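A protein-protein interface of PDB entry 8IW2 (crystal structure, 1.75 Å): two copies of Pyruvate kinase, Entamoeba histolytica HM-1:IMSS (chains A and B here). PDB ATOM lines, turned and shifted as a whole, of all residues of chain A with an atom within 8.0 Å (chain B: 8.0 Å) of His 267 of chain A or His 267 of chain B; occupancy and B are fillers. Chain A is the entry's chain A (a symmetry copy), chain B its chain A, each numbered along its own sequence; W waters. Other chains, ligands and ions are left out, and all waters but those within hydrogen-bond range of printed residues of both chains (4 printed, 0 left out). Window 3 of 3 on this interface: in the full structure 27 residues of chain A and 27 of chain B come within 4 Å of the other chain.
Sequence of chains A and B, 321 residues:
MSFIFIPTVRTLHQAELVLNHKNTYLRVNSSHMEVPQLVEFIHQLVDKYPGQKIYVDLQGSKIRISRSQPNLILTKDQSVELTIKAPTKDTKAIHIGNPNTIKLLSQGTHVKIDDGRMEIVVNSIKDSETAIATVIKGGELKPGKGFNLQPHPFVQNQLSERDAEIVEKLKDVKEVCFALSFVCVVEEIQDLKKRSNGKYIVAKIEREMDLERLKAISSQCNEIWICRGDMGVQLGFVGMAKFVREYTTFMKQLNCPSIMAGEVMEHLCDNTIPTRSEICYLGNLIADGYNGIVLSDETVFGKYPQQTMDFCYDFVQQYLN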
ATOM      1  N   GLU A 263      17.652   5.875  -2.449  1.00  0.00           N
ATOM      2  CA  GLU A 263      18.183   4.792  -3.276  1.00  0.00           C
ATOM      3  C   GLU A 263      18.507   5.251  -4.688  1.00  0.00           C
ATOM      4  O   GLU A 263      18.223   4.501  -5.643  1.00  0.00           O
ATOM      5  CB  GLU A 263      17.207   3.621  -3.291  1.00  0.00           C
ATOM      6  CG  GLU A 263      17.203   2.913  -1.963  1.00  0.00           C
ATOM      7  CD  GLU A 263      16.409   1.642  -1.885  1.00  0.00           C
ATOM      8  OE1 GLU A 263      15.959   1.119  -2.917  1.00  0.00           O
ATOM      9  OE2 GLU A 263      16.237   1.141  -0.765  1.00  0.00           O
ATOM     10  N   VAL A 264      19.163   6.433  -4.819  1.00  0.00           N
ATOM     11  CA  VAL A 264      19.528   6.875  -6.167  1.00  0.00           C
ATOM     12  C   VAL A 264      20.561   5.917  -6.728  1.00  0.00           C
ATOM     13  O   VAL A 264      20.559   5.574  -7.905  1.00  0.00           O
ATOM     14  CB  VAL A 264      19.995   8.351  -6.171  1.00  0.00           C
ATOM     15  CG1 VAL A 264      20.484   8.800  -7.535  1.00  0.00           C
ATOM     16  CG2 VAL A 264      18.885   9.259  -5.752  1.00  0.00           C
ATOM     17  N   MET A 265      21.422   5.410  -5.861  1.00  0.00           N
ATOM     18  CA  MET A 265      22.521   4.571  -6.295  1.00  0.00           C
ATOM     19  C   MET A 265      22.715   3.427  -5.278  1.00  0.00           C
ATOM     20  O   MET A 265      23.845   3.064  -4.924  1.00  0.00           O
ATOM     21  CB  MET A 265      23.791   5.446  -6.500  1.00  0.00           C
ATOM     22  CG  MET A 265      23.619   6.616  -7.490  1.00  0.00           C
ATOM     23  SD  MET A 265      23.240   6.032  -9.383  1.00  0.00           S
ATOM     24  CE  MET A 265      24.649   4.950  -9.193  1.00  0.00           C
ATOM     25  N   GLU A 266      21.603   2.785  -4.878  1.00  0.00           N
ATOM     26  CA  GLU A 266      21.590   1.773  -3.815  1.00  0.00           C
ATOM     27  C   GLU A 266      22.522   0.603  -4.169  1.00  0.00           C
ATOM     28  O   GLU A 266      23.116  -0.003  -3.277  1.00  0.00           O
ATOM     29  CB  GLU A 266      20.136   1.301  -3.635  1.00  0.00           C
ATOM     30  CG  GLU A 266      19.924   0.111  -2.716  1.00  0.00           C
ATOM     31  CD  GLU A 266      20.255   0.388  -1.250  1.00  0.00           C
ATOM     32  OE1 GLU A 266      20.421   1.585  -0.837  1.00  0.00           O
ATOM     33  OE2 GLU A 266      20.401  -0.619  -0.536  1.00  0.00           O
ATOM     34  N   HIS A 267      22.598   0.211  -5.449  1.00  0.00           N
ATOM     35  CA  HIS A 267      23.381  -0.953  -5.834  1.00  0.00           C
ATOM     36  C   HIS A 267      24.855  -0.730  -5.578  1.00  0.00           C
ATOM     37  O   HIS A 267      25.580  -1.738  -5.387  1.00  0.00           O
ATOM     38  CB  HIS A 267      23.216  -1.274  -7.314  1.00  0.00           C
ATOM     39  CG  HIS A 267      23.599  -2.641  -7.708  1.00  0.00           C
ATOM     40  ND1 HIS A 267      22.879  -3.761  -7.344  1.00  0.00           N
ATOM     41  CD2 HIS A 267      24.617  -3.056  -8.516  1.00  0.00           C
ATOM     42  CE1 HIS A 267      23.449  -4.821  -7.935  1.00  0.00           C
ATOM     43  NE2 HIS A 267      24.480  -4.418  -8.659  1.00  0.00           N
ATOM     44  N   LEU A 268      25.281   0.544  -5.467  1.00  0.00           N
ATOM     45  CA  LEU A 268      26.654   0.896  -5.085  1.00  0.00           C
ATOM     46  C   LEU A 268      26.988   0.824  -3.576  1.00  0.00           C
ATOM     47  O   LEU A 268      28.139   1.089  -3.230  1.00  0.00           O
ATOM     48  CB  LEU A 268      27.034   2.271  -5.614  1.00  0.00           C
ATOM     49  CG  LEU A 268      27.214   2.357  -7.132  1.00  0.00           C
ATOM     50  CD1 LEU A 268      27.537   3.782  -7.480  1.00  0.00           C
ATOM     51  CD2 LEU A 268      28.302   1.396  -7.616  1.00  0.00           C
ATOM     52  N   CYS A 269      26.045   0.460  -2.711  1.00  0.00           N
ATOM     53  CA  CYS A 269      26.352   0.196  -1.310  1.00  0.00           C
ATOM     54  C   CYS A 269      27.300  -0.991  -1.180  1.00  0.00           C
ATOM     55  O   CYS A 269      28.198  -0.965  -0.334  1.00  0.00           O
ATOM     56  CB  CYS A 269      25.127  -0.203  -0.523  1.00  0.00           C
ATOM     57  SG  CYS A 269      24.046   1.210  -0.281  1.00  0.00           S
ATOM     58  N   ASP A 270      26.991  -2.016  -1.997  1.00  0.00           N
ATOM     59  CA  ASP A 270      27.595  -3.329  -1.930  1.00  0.00           C
ATOM     60  C   ASP A 270      28.353  -3.655  -3.212  1.00  0.00           C
ATOM     61  O   ASP A 270      29.195  -4.540  -3.190  1.00  0.00           O
ATOM     62  CB  ASP A 270      26.513  -4.375  -1.746  1.00  0.00           C
ATOM     63  CG  ASP A 270      26.281  -4.716  -0.291  1.00  0.00           C
ATOM     64  OD1 ASP A 270      25.696  -3.872   0.451  1.00  0.00           O
ATOM     65  OD2 ASP A 270      26.714  -5.811   0.091  1.00  0.00           O
ATOM     66  N   ASN A 271      28.036  -3.000  -4.332  1.00  0.00           N
ATOM     67  CA  ASN A 271      28.605  -3.400  -5.616  1.00  0.00           C
ATOM     68  C   ASN A 271      29.451  -2.285  -6.194  1.00  0.00           C
ATOM     69  O   ASN A 271      29.408  -1.133  -5.728  1.00  0.00           O
ATOM     70  CB  ASN A 271      27.549  -3.853  -6.608  1.00  0.00           C
ATOM     71  CG  ASN A 271      26.681  -4.953  -6.056  1.00  0.00           C
ATOM     72  OD1 ASN A 271      26.973  -6.126  -6.258  1.00  0.00           O
ATOM     73  ND2 ASN A 271      25.551  -4.609  -5.459  1.00  0.00           N
ATOM     74  N   THR A 272      30.277  -2.679  -7.184  1.00  0.00           N
ATOM     75  CA  THR A 272      31.304  -1.802  -7.734  1.00  0.00           C
ATOM     76  C   THR A 272      30.796  -1.014  -8.956  1.00  0.00           C
ATOM     77  O   THR A 272      31.305   0.062  -9.231  1.00  0.00           O
ATOM     78  CB  THR A 272      32.579  -2.623  -8.066  1.00  0.00           C
ATOM     79  OG1 THR A 272      32.230  -3.653  -8.983  1.00  0.00           O
ATOM     80  CG2 THR A 272      33.196  -3.365  -6.895  1.00  0.00           C
ATOM     81  N   ILE A 273      29.773  -1.545  -9.670  1.00  0.00           N
ATOM     82  CA  ILE A 273      29.227  -0.897 -10.865  1.00  0.00           C
ATOM     83  C   ILE A 273      27.743  -0.613 -10.609  1.00  0.00           C
ATOM     84  O   ILE A 273      27.008  -1.522 -10.306  1.00  0.00           O
ATOM     85  CB  ILE A 273      29.445  -1.839 -12.084  1.00  0.00           C
ATOM     86  CG1 ILE A 273      30.903  -2.303 -12.193  1.00  0.00           C
ATOM     87  CG2 ILE A 273      29.033  -1.163 -13.383  1.00  0.00           C
ATOM     88  CD1 ILE A 273      31.132  -3.408 -13.233  1.00  0.00           C
ATOM     89  N   PRO A 274      27.204   0.592 -10.901  1.00  0.00           N
ATOM     90  CA  PRO A 274      25.743   0.779 -10.805  1.00  0.00           C
ATOM     91  C   PRO A 274      25.043  -0.022 -11.898  1.00  0.00           C
ATOM     92  O   PRO A 274      25.676  -0.335 -12.904  1.00  0.00           O
ATOM     93  CB  PRO A 274      25.617   2.303 -10.895  1.00  0.00           C
ATOM     94  CG  PRO A 274      26.800   2.706 -11.801  1.00  0.00           C
ATOM     95  CD  PRO A 274      27.904   1.733 -11.476  1.00  0.00           C
ATOM     96  N   THR A 275      23.708  -0.286 -11.768  1.00  0.00           N
ATOM     97  CA  THR A 275      23.017  -1.109 -12.746  1.00  0.00           C
ATOM     98  C   THR A 275      22.693  -0.187 -13.942  1.00  0.00           C
ATOM     99  O   THR A 275      22.743   1.051 -13.760  1.00  0.00           O
ATOM    100  CB  THR A 275      21.696  -1.660 -12.233  1.00  0.00           C
ATOM    101  OG1 THR A 275      20.672  -0.644 -12.208  1.00  0.00           O
ATOM    102  CG2 THR A 275      21.821  -2.227 -10.839  1.00  0.00           C
ATOM    103  N   ARG A 276      22.320  -0.797 -15.071  1.00  0.00           N
ATOM    104  CA  ARG A 276      22.030   0.006 -16.248  1.00  0.00           C
ATOM    105  C   ARG A 276      20.800   0.870 -15.969  1.00  0.00           C
ATOM    106  O   ARG A 276      20.743   1.945 -16.535  1.00  0.00           O
ATOM    107  CB  ARG A 276      21.784  -0.856 -17.489  1.00  0.00           C
ATOM    108  CG  ARG A 276      22.972  -1.710 -17.921  1.00  0.00           C
ATOM    109  CD  ARG A 276      24.184  -0.863 -18.092  1.00  0.00           C
ATOM    110  NE  ARG A 276      25.147  -1.520 -18.954  1.00  0.00           N
ATOM    111  CZ  ARG A 276      26.405  -1.794 -18.618  1.00  0.00           C
ATOM    112  NH1 ARG A 276      26.890  -1.437 -17.424  1.00  0.00           N
ATOM    113  NH2 ARG A 276      27.191  -2.350 -19.519  1.00  0.00           N
ATOM    114  N   GLU A 278      19.909   2.150 -12.916  1.00  0.00           N
ATOM    115  CA  GLU A 278      20.415   3.245 -12.110  1.00  0.00           C
ATOM    116  C   GLU A 278      21.015   4.364 -12.971  1.00  0.00           C
ATOM    117  O   GLU A 278      20.772   5.560 -12.725  1.00  0.00           O
ATOM    118  CB  GLU A 278      21.456   2.729 -11.113  1.00  0.00           C
ATOM    119  CG  GLU A 278      20.765   1.963  -9.992  1.00  0.00           C
ATOM    120  CD  GLU A 278      21.715   1.438  -8.944  1.00  0.00           C
ATOM    121  OE1 GLU A 278      22.837   1.037  -9.367  1.00  0.00           O
ATOM    122  OE2 GLU A 278      21.394   1.550  -7.707  1.00  0.00           O
ATOM    123  N   GLU A 298      24.330   4.950   0.509  1.00  0.00           N
ATOM    124  CA  GLU A 298      25.444   4.759  -0.402  1.00  0.00           C
ATOM    125  C   GLU A 298      26.749   5.354   0.136  1.00  0.00           C
ATOM    126  O   GLU A 298      27.800   4.825  -0.184  1.00  0.00           O
ATOM    127  CB  GLU A 298      25.226   5.432  -1.788  1.00  0.00           C
ATOM    128  CG  GLU A 298      23.943   5.108  -2.515  1.00  0.00           C
ATOM    129  CD  GLU A 298      22.687   5.917  -2.248  1.00  0.00           C
ATOM    130  OE1 GLU A 298      22.437   6.315  -1.097  1.00  0.00           O
ATOM    131  OE2 GLU A 298      21.932   6.176  -3.238  1.00  0.00           O
ATOM    132  N   TYR A 304      31.724   1.933  -0.480  1.00  0.00           N
ATOM    133  CA  TYR A 304      32.487   2.711  -1.455  1.00  0.00           C
ATOM    134  C   TYR A 304      32.077   4.194  -1.444  1.00  0.00           C
ATOM    135  O   TYR A 304      31.823   4.765  -2.514  1.00  0.00           O
ATOM    136  CB  TYR A 304      32.340   2.096  -2.859  1.00  0.00           C
ATOM    137  CG  TYR A 304      32.709   0.624  -2.947  1.00  0.00           C
ATOM    138  CD1 TYR A 304      33.970   0.160  -2.589  1.00  0.00           C
ATOM    139  CD2 TYR A 304      31.767  -0.303  -3.344  1.00  0.00           C
ATOM    140  CE1 TYR A 304      34.263  -1.199  -2.631  1.00  0.00           C
ATOM    141  CE2 TYR A 304      32.034  -1.662  -3.375  1.00  0.00           C
ATOM    142  CZ  TYR A 304      33.289  -2.113  -2.997  1.00  0.00           C
ATOM    143  OH  TYR A 304      33.482  -3.471  -3.016  1.00  0.00           O
ATOM    144  N   THR A 308      31.604   6.229  -4.898  1.00  0.00           N
ATOM    145  CA  THR A 308      30.214   6.496  -5.285  1.00  0.00           C
ATOM    146  C   THR A 308      30.040   7.986  -5.596  1.00  0.00           C
ATOM    147  O   THR A 308      29.536   8.372  -6.676  1.00  0.00           O
ATOM    148  CB  THR A 308      29.228   6.003  -4.227  1.00  0.00           C
ATOM    149  OG1 THR A 308      29.425   4.590  -4.097  1.00  0.00           O
ATOM    150  CG2 THR A 308      27.789   6.352  -4.599  1.00  0.00           C
ATOM    151  N   GLU B 263      19.741  -5.476 -17.687  1.00  0.00           N
ATOM    152  CA  GLU B 263      19.719  -5.078 -16.280  1.00  0.00           C
ATOM    153  C   GLU B 263      18.469  -4.290 -15.924  1.00  0.00           C
ATOM    154  O   GLU B 263      18.576  -3.302 -15.170  1.00  0.00           O
ATOM    155  CB  GLU B 263      20.978  -4.289 -15.941  1.00  0.00           C
ATOM    156  CG  GLU B 263      22.180  -5.196 -15.903  1.00  0.00           C
ATOM    157  CD  GLU B 263      23.464  -4.584 -15.422  1.00  0.00           C
ATOM    158  OE1 GLU B 263      23.465  -3.457 -14.902  1.00  0.00           O
ATOM    159  OE2 GLU B 263      24.500  -5.249 -15.556  1.00  0.00           O
ATOM    160  N   VAL B 264      17.285  -4.760 -16.395  1.00  0.00           N
ATOM    161  CA  VAL B 264      16.061  -4.045 -16.027  1.00  0.00           C
ATOM    162  C   VAL B 264      15.847  -4.189 -14.533  1.00  0.00           C
ATOM    163  O   VAL B 264      15.420  -3.269 -13.845  1.00  0.00           O
ATOM    164  CB  VAL B 264      14.853  -4.523 -16.869  1.00  0.00           C
ATOM    165  CG1 VAL B 264      13.551  -3.877 -16.432  1.00  0.00           C
ATOM    166  CG2 VAL B 264      15.061  -4.216 -18.316  1.00  0.00           C
ATOM    167  N   MET B 265      16.216  -5.341 -13.996  1.00  0.00           N
ATOM    168  CA  MET B 265      15.959  -5.637 -12.601  1.00  0.00           C
ATOM    169  C   MET B 265      17.172  -6.389 -12.013  1.00  0.00           C
ATOM    170  O   MET B 265      17.025  -7.349 -11.246  1.00  0.00           O
ATOM    171  CB  MET B 265      14.620  -6.418 -12.475  1.00  0.00           C
ATOM    172  CG  MET B 265      13.394  -5.705 -13.079  1.00  0.00           C
ATOM    173  SD  MET B 265      12.922  -3.974 -12.158  1.00  0.00           S
ATOM    174  CE  MET B 265      13.011  -4.911 -10.638  1.00  0.00           C
ATOM    175  N   GLU B 266      18.385  -5.883 -12.297  1.00  0.00           N
ATOM    176  CA  GLU B 266      19.644  -6.549 -11.939  1.00  0.00           C
ATOM    177  C   GLU B 266      19.735  -6.757 -10.419  1.00  0.00           C
ATOM    178  O   GLU B 266      20.320  -7.741  -9.965  1.00  0.00           O
ATOM    179  CB  GLU B 266      20.801  -5.677 -12.459  1.00  0.00           C
ATOM    180  CG  GLU B 266      22.198  -6.083 -12.026  1.00  0.00           C
ATOM    181  CD  GLU B 266      22.659  -7.428 -12.588  1.00  0.00           C
ATOM    182  OE1 GLU B 266      22.019  -7.986 -13.542  1.00  0.00           O
ATOM    183  OE2 GLU B 266      23.638  -7.938 -12.018  1.00  0.00           O
ATOM    184  N   HIS B 267      19.243  -5.805  -9.614  1.00  0.00           N
ATOM    185  CA  HIS B 267      19.389  -5.893  -8.169  1.00  0.00           C
ATOM    186  C   HIS B 267      18.626  -7.075  -7.612  1.00  0.00           C
ATOM    187  O   HIS B 267      19.019  -7.573  -6.528  1.00  0.00           O
ATOM    188  CB  HIS B 267      18.863  -4.641  -7.476  1.00  0.00           C
ATOM    189  CG  HIS B 267      19.343  -4.437  -6.099  1.00  0.00           C
ATOM    190  ND1 HIS B 267      20.647  -4.105  -5.794  1.00  0.00           N
ATOM    191  CD2 HIS B 267      18.643  -4.451  -4.926  1.00  0.00           C
ATOM    192  CE1 HIS B 267      20.721  -3.911  -4.470  1.00  0.00           C
ATOM    193  NE2 HIS B 267      19.526  -4.094  -3.934  1.00  0.00           N
ATOM    194  N   LEU B 268      17.635  -7.586  -8.369  1.00  0.00           N
ATOM    195  CA  LEU B 268      16.911  -8.812  -8.011  1.00  0.00           C
ATOM    196  C   LEU B 268      17.622 -10.150  -8.327  1.00  0.00           C
ATOM    197  O   LEU B 268      17.048 -11.192  -8.015  1.00  0.00           O
ATOM    198  CB  LEU B 268      15.522  -8.828  -8.633  1.00  0.00           C
ATOM    199  CG  LEU B 268      14.532  -7.823  -8.038  1.00  0.00           C
ATOM    200  CD1 LEU B 268      13.240  -7.943  -8.796  1.00  0.00           C
ATOM    201  CD2 LEU B 268      14.333  -8.060  -6.541  1.00  0.00           C
ATOM    202  N   CYS B 269      18.825 -10.135  -8.896  1.00  0.00           N
ATOM    203  CA  CYS B 269      19.616 -11.352  -9.044  1.00  0.00           C
ATOM    204  C   CYS B 269      19.977 -11.929  -7.680  1.00  0.00           C
ATOM    205  O   CYS B 269      19.967 -13.151  -7.513  1.00  0.00           O
ATOM    206  CB  CYS B 269      20.943 -11.089  -9.714  1.00  0.00           C
ATOM    207  SG  CYS B 269      20.708 -10.730 -11.458  1.00  0.00           S
ATOM    208  N   ASP B 270      20.355 -10.995  -6.786  1.00  0.00           N
ATOM    209  CA  ASP B 270      20.940 -11.286  -5.495  1.00  0.00           C
ATOM    210  C   ASP B 270      20.054 -10.786  -4.360  1.00  0.00           C
ATOM    211  O   ASP B 270      20.212 -11.250  -3.240  1.00  0.00           O
ATOM    212  CB  ASP B 270      22.284 -10.591  -5.381  1.00  0.00           C
ATOM    213  CG  ASP B 270      23.431 -11.486  -5.790  1.00  0.00           C
ATOM    214  OD1 ASP B 270      23.592 -11.757  -7.017  1.00  0.00           O
ATOM    215  OD2 ASP B 270      24.138 -11.926  -4.873  1.00  0.00           O
ATOM    216  N   ASN B 271      19.167  -9.820  -4.612  1.00  0.00           N
ATOM    217  CA  ASN B 271      18.424  -9.187  -3.527  1.00  0.00           C
ATOM    218  C   ASN B 271      16.939  -9.440  -3.678  1.00  0.00           C
ATOM    219  O   ASN B 271      16.466  -9.895  -4.733  1.00  0.00           O
ATOM    220  CB  ASN B 271      18.714  -7.700  -3.409  1.00  0.00           C
ATOM    221  CG  ASN B 271      20.187  -7.415  -3.271  1.00  0.00           C
ATOM    222  OD1 ASN B 271      20.692  -7.317  -2.160  1.00  0.00           O
ATOM    223  ND2 ASN B 271      20.874  -7.162  -4.374  1.00  0.00           N
ATOM    224  N   THR B 272      16.224  -9.195  -2.562  1.00  0.00           N
ATOM    225  CA  THR B 272      14.817  -9.560  -2.445  1.00  0.00           C
ATOM    226  C   THR B 272      13.885  -8.408  -2.866  1.00  0.00           C
ATOM    227  O   THR B 272      12.767  -8.663  -3.286  1.00  0.00           O
ATOM    228  CB  THR B 272      14.515 -10.049  -1.003  1.00  0.00           C
ATOM    229  OG1 THR B 272      14.861  -9.015  -0.091  1.00  0.00           O
ATOM    230  CG2 THR B 272      15.333 -11.240  -0.539  1.00  0.00           C
ATOM    231  N   ILE B 273      14.363  -7.142  -2.774  1.00  0.00           N
ATOM    232  CA  ILE B 273      13.558  -5.969  -3.121  1.00  0.00           C
ATOM    233  C   ILE B 273      14.277  -5.222  -4.249  1.00  0.00           C
ATOM    234  O   ILE B 273      15.418  -4.860  -4.089  1.00  0.00           O
ATOM    235  CB  ILE B 273      13.386  -5.090  -1.848  1.00  0.00           C
ATOM    236  CG1 ILE B 273      12.880  -5.908  -0.653  1.00  0.00           C
ATOM    237  CG2 ILE B 273      12.436  -3.930  -2.103  1.00  0.00           C
ATOM    238  CD1 ILE B 273      12.909  -5.152   0.681  1.00  0.00           C
ATOM    239  N   PRO B 274      13.604  -4.793  -5.340  1.00  0.00           N
ATOM    240  CA  PRO B 274      14.286  -3.931  -6.325  1.00  0.00           C
ATOM    241  C   PRO B 274      14.563  -2.562  -5.712  1.00  0.00           C
ATOM    242  O   PRO B 274      13.886  -2.188  -4.759  1.00  0.00           O
ATOM    243  CB  PRO B 274      13.303  -3.961  -7.499  1.00  0.00           C
ATOM    244  CG  PRO B 274      11.929  -4.106  -6.812  1.00  0.00           C
ATOM    245  CD  PRO B 274      12.178  -4.957  -5.593  1.00  0.00           C
ATOM    246  N   THR B 275      15.496  -1.754  -6.303  1.00  0.00           N
ATOM    247  CA  THR B 275      15.847  -0.474  -5.711  1.00  0.00           C
ATOM    248  C   THR B 275      14.748   0.522  -6.140  1.00  0.00           C
ATOM    249  O   THR B 275      14.013   0.207  -7.104  1.00  0.00           O
ATOM    250  CB  THR B 275      17.171   0.072  -6.221  1.00  0.00           C
ATOM    251  OG1 THR B 275      17.047   0.604  -7.556  1.00  0.00           O
ATOM    252  CG2 THR B 275      18.251  -0.984  -6.241  1.00  0.00           C
ATOM    253  N   ARG B 276      14.713   1.681  -5.476  1.00  0.00           N
ATOM    254  CA  ARG B 276      13.684   2.655  -5.803  1.00  0.00           C
ATOM    255  C   ARG B 276      13.906   3.150  -7.233  1.00  0.00           C
ATOM    256  O   ARG B 276      12.918   3.483  -7.858  1.00  0.00           O
ATOM    257  CB  ARG B 276      13.687   3.845  -4.840  1.00  0.00           C
ATOM    258  CG  ARG B 276      13.396   3.490  -3.385  1.00  0.00           C
ATOM    259  CD  ARG B 276      12.123   2.724  -3.282  1.00  0.00           C
ATOM    260  NE  ARG B 276      11.580   2.816  -1.941  1.00  0.00           N
ATOM    261  CZ  ARG B 276      11.300   1.774  -1.163  1.00  0.00           C
ATOM    262  NH1 ARG B 276      11.478   0.522  -1.600  1.00  0.00           N
ATOM    263  NH2 ARG B 276      10.760   1.997   0.019  1.00  0.00           N
ATOM    264  N   GLU B 278      15.218   1.303  -9.805  1.00  0.00           N
ATOM    265  CA  GLU B 278      14.688   0.240 -10.639  1.00  0.00           C
ATOM    266  C   GLU B 278      13.170   0.359 -10.825  1.00  0.00           C
ATOM    267  O   GLU B 278      12.648   0.192 -11.943  1.00  0.00           O
ATOM    268  CB  GLU B 278      15.043  -1.125 -10.043  1.00  0.00           C
ATOM    269  CG  GLU B 278      16.521  -1.419 -10.267  1.00  0.00           C
ATOM    270  CD  GLU B 278      16.956  -2.762  -9.733  1.00  0.00           C
ATOM    271  OE1 GLU B 278      16.408  -3.133  -8.657  1.00  0.00           O
ATOM    272  OE2 GLU B 278      17.734  -3.489 -10.450  1.00  0.00           O
ATOM    273  N   GLU B 298      18.551 -11.946 -14.384  1.00  0.00           N
ATOM    274  CA  GLU B 298      17.599 -11.973 -13.289  1.00  0.00           C
ATOM    275  C   GLU B 298      16.836 -13.299 -13.208  1.00  0.00           C
ATOM    276  O   GLU B 298      16.465 -13.686 -12.113  1.00  0.00           O
ATOM    277  CB  GLU B 298      16.503 -10.875 -13.402  1.00  0.00           C
ATOM    278  CG  GLU B 298      16.971  -9.454 -13.604  1.00  0.00           C
ATOM    279  CD  GLU B 298      17.236  -8.927 -15.002  1.00  0.00           C
ATOM    280  OE1 GLU B 298      17.742  -9.670 -15.862  1.00  0.00           O
ATOM    281  OE2 GLU B 298      16.906  -7.724 -15.250  1.00  0.00           O
ATOM    282  N   TYR B 304      16.176 -15.693  -7.670  1.00  0.00           N
ATOM    283  CA  TYR B 304      14.734 -15.555  -7.469  1.00  0.00           C
ATOM    284  C   TYR B 304      13.981 -15.470  -8.807  1.00  0.00           C
ATOM    285  O   TYR B 304      13.144 -14.572  -8.982  1.00  0.00           O
ATOM    286  CB  TYR B 304      14.434 -14.338  -6.574  1.00  0.00           C
ATOM    287  CG  TYR B 304      15.160 -14.340  -5.238  1.00  0.00           C
ATOM    288  CD1 TYR B 304      15.014 -15.378  -4.325  1.00  0.00           C
ATOM    289  CD2 TYR B 304      16.031 -13.318  -4.922  1.00  0.00           C
ATOM    290  CE1 TYR B 304      15.729 -15.379  -3.132  1.00  0.00           C
ATOM    291  CE2 TYR B 304      16.766 -13.310  -3.748  1.00  0.00           C
ATOM    292  CZ  TYR B 304      16.625 -14.360  -2.855  1.00  0.00           C
ATOM    293  OH  TYR B 304      17.404 -14.311  -1.727  1.00  0.00           O
ATOM    294  N   THR B 308      10.977 -12.822  -9.319  1.00  0.00           N
ATOM    295  CA  THR B 308      11.303 -11.654 -10.146  1.00  0.00           C
ATOM    296  C   THR B 308      10.245 -11.483 -11.241  1.00  0.00           C
ATOM    297  O   THR B 308       9.653 -10.393 -11.411  1.00  0.00           O
ATOM    298  CB  THR B 308      12.719 -11.740 -10.714  1.00  0.00           C
ATOM    299  OG1 THR B 308      13.615 -11.800  -9.597  1.00  0.00           O
ATOM    300  CG2 THR B 308      13.024 -10.562 -11.635  1.00  0.00           C
HETATM  301  O   HOH W   1      19.168   2.348  -7.193  1.00  0.00           O
HETATM  302  O   HOH W   2      18.641  -2.510 -12.469  1.00  0.00           O
HETATM  303  O   HOH W   3      25.611  -1.935 -15.022  1.00  0.00           O
HETATM  304  O   HOH W   4      13.793  -0.375  -2.820  1.00  0.00           O
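A ring nitrogen (ND1) of His 267 of chain B sits at hydrogen-bond distance from a ring nitrogen (ND1) of His 267 of chain A (2.7 Å). N of Arg 276 of chain A lies within hydrogen-bond range of OE1 of Glu 263 of chain B (2.9 Å). The backbone NH (N) of Arg 276 of chain B sits at hydrogen-bond distance from the side-chain carboxylate (OE1) of Glu 263 of chain A (2.9 Å).
The backbone NH (N) of His 267 of chain A lies within hydrogen-bond range of the side-chain carboxylate (OE2) of Glu 278 of chain A, 2.9 Å away. OE2 of Glu 278 of chain B sits at hydrogen-bond distance from N of Glu 266 of chain B, at 3.1 Å. N of Thr 275 of chain B sits at hydrogen-bond distance from OE1 of Glu 278 of chain B (2.9 Å). OE2 of Glu 278 of chain B is in hydrogen-bond range of N of His 267 of chain B, at 2.9 Å.
Among the printed residues, pairs that only touch across the chains: Glu 263 of chain A with Thr 275 of chain B, Thr 275 of chain A with Glu 263 of chain B, Glu 266 of chain A with Thr 275 of chain B and Thr 275 of chain A with Glu 266 of chain B.
Printed residues of chain B within 4 Å of Glu 263 of chain A: Thr 275 and Arg 276. His 267 of chain A touches just one residue of chain B: His 267. Asp 270 of chain A touches none of the printed residues of chain B. Of the printed residues of chain B, Arg 276 of chain A touches Glu 263 (2.9 Å). Of the printed residues of chain A, Glu 263 of chain B touches Thr 275 (3.2 Å) and Arg 276 (2.9 Å). His 267 of chain B touches just one residue of chain A: His 267 (2.7 Å). Of the printed residues of chain A, Arg 276 of chain B touches Glu 263 (2.9 Å). The nearest residue of chain A that does not touch His 267 of chain B is Glu 266 of chain A (4.4 Å). The nearest printed residue of chain A that does not touch Arg 276 of chain B is Glu 266 of chain A (5.7 Å).
Along chain A the printed residues that touch a printed residue of chain B span positions 263 to 276. Among the printed residues, no Asp or Glu carboxylate lies within 4 Å of a Lys or Arg side-chain nitrogen of the other chain.
Glu 263 of chain A touches Arg 276 of chain B, and with the chains exchanged Arg 276 of chain A touches Glu 263 of chain B. Glu 266 of chain A touches Thr 275 of chain B, and with the chains exchanged Thr 275 of chain A touches Glu 266 of chain B. His 267 of chain B touches its own counterpart, His 267 of chain A.
Water W2 lies within hydrogen-bond range of OE2 of Glu 278 of chain B (2.4 Å), OG1 of Thr 275 of chain A (2.8 Å), O of Glu 263 of chain B (2.8 Å) and N of Glu 266 of chain B (3.4 Å). Water W4 lies within hydrogen-bond range of the side-chain carboxylate of Glu 263 of chain A (2.6 Å), the backbone carbonyl oxygen of Pro 274 of chain B (2.7 Å) and the guanidinium group of Arg 276 of chain B (2.8 Å).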
